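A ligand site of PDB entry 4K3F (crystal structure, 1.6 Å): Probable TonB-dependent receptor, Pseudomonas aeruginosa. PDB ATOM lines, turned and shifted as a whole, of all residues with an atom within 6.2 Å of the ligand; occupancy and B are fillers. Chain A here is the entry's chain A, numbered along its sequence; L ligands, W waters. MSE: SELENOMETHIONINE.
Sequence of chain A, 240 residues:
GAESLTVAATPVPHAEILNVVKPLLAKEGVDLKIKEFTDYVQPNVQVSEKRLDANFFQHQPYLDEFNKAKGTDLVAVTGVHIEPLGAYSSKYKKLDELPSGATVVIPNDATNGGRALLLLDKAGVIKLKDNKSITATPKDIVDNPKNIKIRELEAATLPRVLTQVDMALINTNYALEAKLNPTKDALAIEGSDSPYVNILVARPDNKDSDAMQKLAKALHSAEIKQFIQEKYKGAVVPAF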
ATOM      1  N   THR A  10     -12.916  -4.709  16.360  1.00  0.00           N
ATOM      2  CA  THR A  10     -11.674  -5.485  16.292  1.00  0.00           C
ATOM      3  C   THR A  10     -11.316  -5.868  17.751  1.00  0.00           C
ATOM      4  O   THR A  10     -11.767  -5.267  18.739  1.00  0.00           O
ATOM      5  CB  THR A  10     -10.507  -4.714  15.606  1.00  0.00           C
ATOM      6  OG1 THR A  10     -10.569  -3.331  16.017  1.00  0.00           O
ATOM      7  CG2 THR A  10     -10.680  -4.764  14.084  1.00  0.00           C
ATOM      8  N   PRO A  13      -7.621  -2.780  20.695  1.00  0.00           N
ATOM      9  CA  PRO A  13      -8.242  -2.547  21.989  1.00  0.00           C
ATOM     10  C   PRO A  13      -9.758  -2.529  22.004  1.00  0.00           C
ATOM     11  O   PRO A  13     -10.344  -2.527  23.088  1.00  0.00           O
ATOM     12  CB  PRO A  13      -7.714  -1.156  22.371  1.00  0.00           C
ATOM     13  CG  PRO A  13      -7.636  -0.457  21.066  1.00  0.00           C
ATOM     14  CD  PRO A  13      -7.065  -1.514  20.134  1.00  0.00           C
ATOM     15  N   HIS A  14     -10.402  -2.504  20.819  1.00  0.00           N
ATOM     16  CA  HIS A  14     -11.793  -2.075  20.747  1.00  0.00           C
ATOM     17  C   HIS A  14     -12.760  -2.953  21.508  1.00  0.00           C
ATOM     18  O   HIS A  14     -13.564  -2.458  22.290  1.00  0.00           O
ATOM     19  CB  HIS A  14     -12.224  -1.929  19.278  1.00  0.00           C
ATOM     20  CG  HIS A  14     -11.275  -1.085  18.488  1.00  0.00           C
ATOM     21  ND1 HIS A  14     -10.003  -1.499  18.165  1.00  0.00           N
ATOM     22  CD2 HIS A  14     -11.394   0.172  18.023  1.00  0.00           C
ATOM     23  CE1 HIS A  14      -9.381  -0.526  17.507  1.00  0.00           C
ATOM     24  NE2 HIS A  14     -10.217   0.500  17.406  1.00  0.00           N
ATOM     25  N   TYR A  40     -10.885  -5.160   8.417  1.00  0.00           N
ATOM     26  CA  TYR A  40     -11.263  -3.783   8.317  1.00  0.00           C
ATOM     27  C   TYR A  40     -12.428  -3.515   7.338  1.00  0.00           C
ATOM     28  O   TYR A  40     -12.775  -2.372   7.086  1.00  0.00           O
ATOM     29  CB  TYR A  40     -10.053  -2.989   7.854  1.00  0.00           C
ATOM     30  CG  TYR A  40      -8.960  -2.655   8.874  1.00  0.00           C
ATOM     31  CD1 TYR A  40      -9.110  -2.882  10.236  1.00  0.00           C
ATOM     32  CD2 TYR A  40      -7.775  -2.075   8.425  1.00  0.00           C
ATOM     33  CE1 TYR A  40      -8.100  -2.508  11.133  1.00  0.00           C
ATOM     34  CE2 TYR A  40      -6.805  -1.679   9.301  1.00  0.00           C
ATOM     35  CZ  TYR A  40      -6.936  -1.896  10.660  1.00  0.00           C
ATOM     36  OH  TYR A  40      -5.910  -1.479  11.511  1.00  0.00           O
ATOM     37  N   PHE A  57     -13.867   0.413  15.291  1.00  0.00           N
ATOM     38  CA  PHE A  57     -12.632  -0.169  14.708  1.00  0.00           C
ATOM     39  C   PHE A  57     -11.828   0.763  13.838  1.00  0.00           C
ATOM     40  O   PHE A  57     -10.710   0.435  13.551  1.00  0.00           O
ATOM     41  CB  PHE A  57     -12.881  -1.455  13.906  1.00  0.00           C
ATOM     42  CG  PHE A  57     -13.343  -1.222  12.484  1.00  0.00           C
ATOM     43  CD1 PHE A  57     -14.632  -0.848  12.224  1.00  0.00           C
ATOM     44  CD2 PHE A  57     -12.444  -1.330  11.431  1.00  0.00           C
ATOM     45  CE1 PHE A  57     -15.065  -0.634  10.886  1.00  0.00           C
ATOM     46  CE2 PHE A  57     -12.864  -1.118  10.133  1.00  0.00           C
ATOM     47  CZ  PHE A  57     -14.165  -0.759   9.873  1.00  0.00           C
ATOM     48  N   GLN A  58     -12.382   1.874  13.365  1.00  0.00           N
ATOM     49  CA  GLN A  58     -11.726   2.661  12.276  1.00  0.00           C
ATOM     50  C   GLN A  58     -11.581   4.106  12.690  1.00  0.00           C
ATOM     51  O   GLN A  58     -12.179   4.541  13.690  1.00  0.00           O
ATOM     52  CB  GLN A  58     -12.548   2.569  10.986  1.00  0.00           C
ATOM     53  CG  GLN A  58     -13.820   3.436  11.034  1.00  0.00           C
ATOM     54  CD  GLN A  58     -14.845   2.938  10.047  1.00  0.00           C
ATOM     55  OE1 GLN A  58     -14.601   2.854   8.832  1.00  0.00           O
ATOM     56  NE2 GLN A  58     -15.970   2.512  10.558  1.00  0.00           N
ATOM     57  N   HIS A  59     -10.778   4.848  11.926  1.00  0.00           N
ATOM     58  CA  HIS A  59     -10.679   6.274  12.086  1.00  0.00           C
ATOM     59  C   HIS A  59     -11.497   6.956  10.981  1.00  0.00           C
ATOM     60  O   HIS A  59     -12.034   6.320  10.083  1.00  0.00           O
ATOM     61  CB  HIS A  59      -9.217   6.766  12.114  1.00  0.00           C
ATOM     62  CG  HIS A  59      -8.318   6.180  11.029  1.00  0.00           C
ATOM     63  ND1 HIS A  59      -8.541   6.391   9.665  1.00  0.00           N
ATOM     64  CD2 HIS A  59      -7.219   5.405  11.107  1.00  0.00           C
ATOM     65  CE1 HIS A  59      -7.593   5.783   8.965  1.00  0.00           C
ATOM     66  NE2 HIS A  59      -6.762   5.189   9.826  1.00  0.00           N
ATOM     67  N   TYR A  62     -10.506   6.711   7.183  1.00  0.00           N
ATOM     68  CA  TYR A  62     -10.845   5.384   6.651  1.00  0.00           C
ATOM     69  C   TYR A  62     -12.344   5.287   6.340  1.00  0.00           C
ATOM     70  O   TYR A  62     -12.738   4.822   5.250  1.00  0.00           O
ATOM     71  CB  TYR A  62     -10.415   4.279   7.643  1.00  0.00           C
ATOM     72  CG  TYR A  62     -10.652   2.908   7.099  1.00  0.00           C
ATOM     73  CD1 TYR A  62     -11.871   2.291   7.249  1.00  0.00           C
ATOM     74  CD2 TYR A  62      -9.654   2.237   6.354  1.00  0.00           C
ATOM     75  CE1 TYR A  62     -12.105   1.046   6.733  1.00  0.00           C
ATOM     76  CE2 TYR A  62      -9.881   0.974   5.828  1.00  0.00           C
ATOM     77  CZ  TYR A  62     -11.096   0.389   6.012  1.00  0.00           C
ATOM     78  OH  TYR A  62     -11.329  -0.865   5.446  1.00  0.00           O
ATOM     79  N   HIS A  81     -10.272   7.067  21.007  1.00  0.00           N
ATOM     80  CA  HIS A  81      -8.863   6.930  21.281  1.00  0.00           C
ATOM     81  C   HIS A  81      -8.043   7.048  20.030  1.00  0.00           C
ATOM     82  O   HIS A  81      -8.575   6.987  18.916  1.00  0.00           O
ATOM     83  CB  HIS A  81      -8.554   5.587  21.970  1.00  0.00           C
ATOM     84  CG  HIS A  81      -8.709   4.400  21.070  1.00  0.00           C
ATOM     85  ND1 HIS A  81      -9.842   3.627  20.998  1.00  0.00           N
ATOM     86  CD2 HIS A  81      -7.847   3.855  20.176  1.00  0.00           C
ATOM     87  CE1 HIS A  81      -9.669   2.662  20.118  1.00  0.00           C
ATOM     88  NE2 HIS A  81      -8.465   2.790  19.594  1.00  0.00           N
ATOM     89  N   ILE A  82      -6.748   7.221  20.232  1.00  0.00           N
ATOM     90  CA  ILE A  82      -5.789   7.265  19.116  1.00  0.00           C
ATOM     91  C   ILE A  82      -4.827   6.111  19.334  1.00  0.00           C
ATOM     92  O   ILE A  82      -4.497   5.776  20.492  1.00  0.00           O
ATOM     93  CB  ILE A  82      -5.003   8.611  19.049  1.00  0.00           C
ATOM     94  CG1 ILE A  82      -5.973   9.792  19.040  1.00  0.00           C
ATOM     95  CG2 ILE A  82      -4.132   8.698  17.823  1.00  0.00           C
ATOM     96  CD1 ILE A  82      -5.864  10.649  20.282  1.00  0.00           C
ATOM     97  N   GLU A  83      -4.358   5.517  18.239  1.00  0.00           N
ATOM     98  CA  GLU A  83      -3.365   4.419  18.274  1.00  0.00           C
ATOM     99  C   GLU A  83      -2.172   4.842  17.449  1.00  0.00           C
ATOM    100  O   GLU A  83      -2.089   4.510  16.276  1.00  0.00           O
ATOM    101  CB  GLU A  83      -3.951   3.152  17.609  1.00  0.00           C
ATOM    102  CG  GLU A  83      -5.095   2.540  18.338  1.00  0.00           C
ATOM    103  CD  GLU A  83      -5.784   1.407  17.584  1.00  0.00           C
ATOM    104  OE1 GLU A  83      -5.227   0.808  16.602  1.00  0.00           O
ATOM    105  OE2 GLU A  83      -6.900   1.126  17.967  1.00  0.00           O
ATOM    106  N   LEU A  85       0.713   5.082  15.181  1.00  0.00           N
ATOM    107  CA  LEU A  85       1.234   4.009  14.319  1.00  0.00           C
ATOM    108  C   LEU A  85       2.755   3.962  14.427  1.00  0.00           C
ATOM    109  O   LEU A  85       3.424   5.008  14.295  1.00  0.00           O
ATOM    110  CB  LEU A  85       0.816   4.282  12.895  1.00  0.00           C
ATOM    111  CG  LEU A  85       1.143   3.073  12.008  1.00  0.00           C
ATOM    112  CD1 LEU A  85      -0.084   2.629  11.291  1.00  0.00           C
ATOM    113  CD2 LEU A  85       2.240   3.506  11.098  1.00  0.00           C
ATOM    114  N   ASP A 109      -4.376  -0.001   1.836  1.00  0.00           N
ATOM    115  CA  ASP A 109      -5.580   0.825   1.716  1.00  0.00           C
ATOM    116  C   ASP A 109      -5.178   2.328   1.688  1.00  0.00           C
ATOM    117  O   ASP A 109      -4.132   2.722   2.179  1.00  0.00           O
ATOM    118  CB  ASP A 109      -6.587   0.572   2.847  1.00  0.00           C
ATOM    119  CG  ASP A 109      -6.045   0.907   4.171  1.00  0.00           C
ATOM    120  OD1 ASP A 109      -5.223   0.139   4.713  1.00  0.00           O
ATOM    121  OD2 ASP A 109      -6.424   1.955   4.705  1.00  0.00           O
ATOM    122  N   THR A 111      -5.962   5.279   3.077  1.00  0.00           N
ATOM    123  CA  THR A 111      -5.675   6.125   4.236  1.00  0.00           C
ATOM    124  C   THR A 111      -4.582   5.584   5.144  1.00  0.00           C
ATOM    125  O   THR A 111      -3.765   6.349   5.620  1.00  0.00           O
ATOM    126  CB  THR A 111      -6.925   6.506   5.041  1.00  0.00           C
ATOM    127  OG1 THR A 111      -7.542   5.339   5.630  1.00  0.00           O
ATOM    128  CG2 THR A 111      -7.922   7.177   4.126  1.00  0.00           C
ATOM    129  N   ASN A 112      -4.546   4.296   5.399  1.00  0.00           N
ATOM    130  CA  ASN A 112      -3.466   3.760   6.222  1.00  0.00           C
ATOM    131  C   ASN A 112      -2.121   3.673   5.477  1.00  0.00           C
ATOM    132  O   ASN A 112      -1.065   3.824   6.106  1.00  0.00           O
ATOM    133  CB  ASN A 112      -3.883   2.471   6.903  1.00  0.00           C
ATOM    134  CG  ASN A 112      -4.969   2.687   7.899  1.00  0.00           C
ATOM    135  OD1 ASN A 112      -4.778   3.309   8.959  1.00  0.00           O
ATOM    136  ND2 ASN A 112      -6.112   2.150   7.594  1.00  0.00           N
ATOM    137  N   ARG A 115      -0.989   7.400   5.553  1.00  0.00           N
ATOM    138  CA  ARG A 115      -0.539   7.600   6.914  1.00  0.00           C
ATOM    139  C   ARG A 115       0.884   7.051   7.166  1.00  0.00           C
ATOM    140  O   ARG A 115       1.724   7.708   7.773  1.00  0.00           O
ATOM    141  CB  ARG A 115      -1.543   6.922   7.815  1.00  0.00           C
ATOM    142  CG  ARG A 115      -1.170   6.764   9.234  1.00  0.00           C
ATOM    143  CD  ARG A 115      -2.256   5.965   9.923  1.00  0.00           C
ATOM    144  NE  ARG A 115      -2.144   6.166  11.334  1.00  0.00           N
ATOM    145  CZ  ARG A 115      -2.932   5.595  12.242  1.00  0.00           C
ATOM    146  NH1 ARG A 115      -3.863   4.721  11.868  1.00  0.00           N
ATOM    147  NH2 ARG A 115      -2.734   5.883  13.495  1.00  0.00           N
ATOM    148  N   ASN A 171      -0.518  -1.110  11.882  1.00  0.00           N
ATOM    149  CA  ASN A 171      -1.579  -0.534  12.681  1.00  0.00           C
ATOM    150  C   ASN A 171      -1.523  -1.117  14.073  1.00  0.00           C
ATOM    151  O   ASN A 171      -1.362  -2.349  14.280  1.00  0.00           O
ATOM    152  CB  ASN A 171      -2.952  -0.803  12.080  1.00  0.00           C
ATOM    153  CG  ASN A 171      -3.143  -0.113  10.750  1.00  0.00           C
ATOM    154  OD1 ASN A 171      -2.810  -0.661   9.679  1.00  0.00           O
ATOM    155  ND2 ASN A 171      -3.622   1.112  10.798  1.00  0.00           N
ATOM    156  N   THR A 172      -1.721  -0.258  15.056  1.00  0.00           N
ATOM    157  CA  THR A 172      -1.488  -0.663  16.463  1.00  0.00           C
ATOM    158  C   THR A 172      -2.428  -1.798  16.926  1.00  0.00           C
ATOM    159  O   THR A 172      -2.037  -2.696  17.695  1.00  0.00           O
ATOM    160  CB  THR A 172      -1.585   0.577  17.356  1.00  0.00           C
ATOM    161  OG1 THR A 172      -0.489   1.416  17.011  1.00  0.00           O
ATOM    162  CG2 THR A 172      -1.542   0.206  18.826  1.00  0.00           C
ATOM    163  N   ASN A 173      -3.697  -1.791  16.499  1.00  0.00           N
ATOM    164  CA  ASN A 173      -4.594  -2.875  16.863  1.00  0.00           C
ATOM    165  C   ASN A 173      -4.039  -4.240  16.500  1.00  0.00           C
ATOM    166  O   ASN A 173      -4.048  -5.162  17.321  1.00  0.00           O
ATOM    167  CB  ASN A 173      -6.004  -2.701  16.318  1.00  0.00           C
ATOM    168  CG  ASN A 173      -6.105  -2.904  14.821  1.00  0.00           C
ATOM    169  OD1 ASN A 173      -5.656  -2.076  14.033  1.00  0.00           O
ATOM    170  ND2 ASN A 173      -6.660  -4.025  14.433  1.00  0.00           N
ATOM    171  N   TYR A 196      -6.181  10.554  13.269  1.00  0.00           N
ATOM    172  CA  TYR A 196      -6.571   9.142  13.318  1.00  0.00           C
ATOM    173  C   TYR A 196      -7.275   8.677  14.602  1.00  0.00           C
ATOM    174  O   TYR A 196      -7.211   7.485  14.977  1.00  0.00           O
ATOM    175  CB  TYR A 196      -5.390   8.232  12.978  1.00  0.00           C
ATOM    176  CG  TYR A 196      -4.724   8.650  11.690  1.00  0.00           C
ATOM    177  CD1 TYR A 196      -5.379   8.531  10.462  1.00  0.00           C
ATOM    178  CD2 TYR A 196      -3.477   9.269  11.702  1.00  0.00           C
ATOM    179  CE1 TYR A 196      -4.804   8.937   9.284  1.00  0.00           C
ATOM    180  CE2 TYR A 196      -2.892   9.681  10.511  1.00  0.00           C
ATOM    181  CZ  TYR A 196      -3.560   9.530   9.322  1.00  0.00           C
ATOM    182  OH  TYR A 196      -2.970   9.960   8.182  1.00  0.00           O
ATOM    183  N   VAL A 197      -8.042   9.558  15.217  1.00  0.00           N
ATOM    184  CA  VAL A 197      -8.878   9.128  16.314  1.00  0.00           C
ATOM    185  C   VAL A 197      -9.827   8.042  15.839  1.00  0.00           C
ATOM    186  O   VAL A 197     -10.419   8.131  14.762  1.00  0.00           O
ATOM    187  CB  VAL A 197      -9.672  10.309  16.890  1.00  0.00           C
ATOM    188  CG1 VAL A 197     -10.654   9.860  17.943  1.00  0.00           C
ATOM    189  CG2 VAL A 197      -8.741  11.379  17.422  1.00  0.00           C
ATOM    190  N   ASN A 198      -9.899   6.955  16.606  1.00  0.00           N
ATOM    191  CA  ASN A 198     -10.850   5.867  16.337  1.00  0.00           C
ATOM    192  C   ASN A 198     -12.239   6.233  16.834  1.00  0.00           C
ATOM    193  O   ASN A 198     -12.392   6.773  17.924  1.00  0.00           O
ATOM    194  CB  ASN A 198     -10.375   4.559  16.977  1.00  0.00           C
ATOM    195  CG  ASN A 198      -9.233   3.891  16.167  1.00  0.00           C
ATOM    196  OD1 ASN A 198      -9.227   2.677  16.006  1.00  0.00           O
ATOM    197  ND2 ASN A 198      -8.313   4.715  15.586  1.00  0.00           N
HETATM  198  N   MSE L   1      -7.229   0.842  14.922  1.00  0.00           N
HETATM  199  CA  MSE L   1      -6.673   1.187  13.578  1.00  0.00           C
HETATM  200  C   MSE L   1      -5.762   2.393  13.784  1.00  0.00           C
HETATM  201  O   MSE L   1      -6.132   3.327  14.498  1.00  0.00           O
HETATM  202  OXT MSE L   1      -4.658   2.439  13.208  1.00  0.00           O
HETATM  203  CB  MSE L   1      -7.782   1.504  12.563  1.00  0.00           C
HETATM  204  CG  MSE L   1      -7.238   1.822  11.190  1.00  0.00           C
HETATM  205 SE   MSE L   1      -8.687   2.384   9.992  1.00  0.00          SE
HETATM  206  CE  MSE L   1      -9.622   0.753   9.829  1.00  0.00           C
HETATM  207  O   HOH W   1      -5.052   5.700  15.397  1.00  0.00           O
HETATM  208  O   HOH W   2      -2.180   2.490  14.316  1.00  0.00           O
HETATM  209  O   HOH W   3      -8.952  -1.450  14.439  1.00  0.00           O
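The side-chain carboxylate (OE1) of Glu 83 lies within salt-bridge range of a nitrogen (N) of the ligand (2.6 Å).
The guanidinium group (NH1) of Arg 115 lies within salt-bridge range of an oxygen (OXT) of the ligand.
The side-chain amide nitrogen of Asn 198 lies within hydrogen-bond range of an oxygen (O) of the ligand.
The side-chain amide nitrogen (ND2) of Asn 171 is in hydrogen-bond range of an oxygen (OXT) of the ligand.
A nitrogen (N) of the ligand sits at hydrogen-bond distance from the side-chain amide oxygen (OD1) of Asn 173 (3.4 Å).
The backbone carbonyl oxygen (O) of Glu 83 is in hydrogen-bond range of the guanidinium group (NH2) of Arg 115, 3.2 Å away.
The side-chain amide oxygen of Asn 198 lies close to the side-chain carboxylate of Glu 83.
OE1 of Glu 83 lies within hydrogen-bond range of N of Asn 173.
The guanidinium group (NH1) of Arg 115 is in hydrogen-bond range of the side-chain amide oxygen (OD1) of Asn 112, 3.4 Å away.
OD1 of Asn 198 is in hydrogen-bond range of NE2 of His 14, 2.8 Å away.
ND2 of Asn 171 sits at hydrogen-bond distance from OD1 of Asn 112 (3.1 Å).
OH of Tyr 40 is in hydrogen-bond range of OD1 of Asn 173.
The backbone carbonyl oxygen (O) of Tyr 40 is in hydrogen-bond range of the side-chain hydroxyl (OH) of Tyr 62, 2.7 Å away.
His 14 touches the ligand (CE1 to N, 3.6 Å).
Tyr 40 touches the ligand.
O of Phe 57 touches CB of the ligand (3.3 Å).
Gln 58 touches the ligand.
NE2 of His 59 touches SE of the ligand, 3.4 Å away.
Tyr 62 touches the ligand.
ND2 of Asn 112 touches SE of the ligand (3.5 Å).
Of the 22 residues printed, 12 come within 4 Å of the ligand.
The nearest printed residue that does not touch the ligand is Tyr 196 (4.3 Å).
Water W2 lies within hydrogen-bond range of OXT of the ligand, O of Glu 83 and N of Thr 172.
Water W3 lies within hydrogen-bond range of O of Phe 57, N of the ligand, OG1 of Thr 10 and OD1 of Asn 173.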
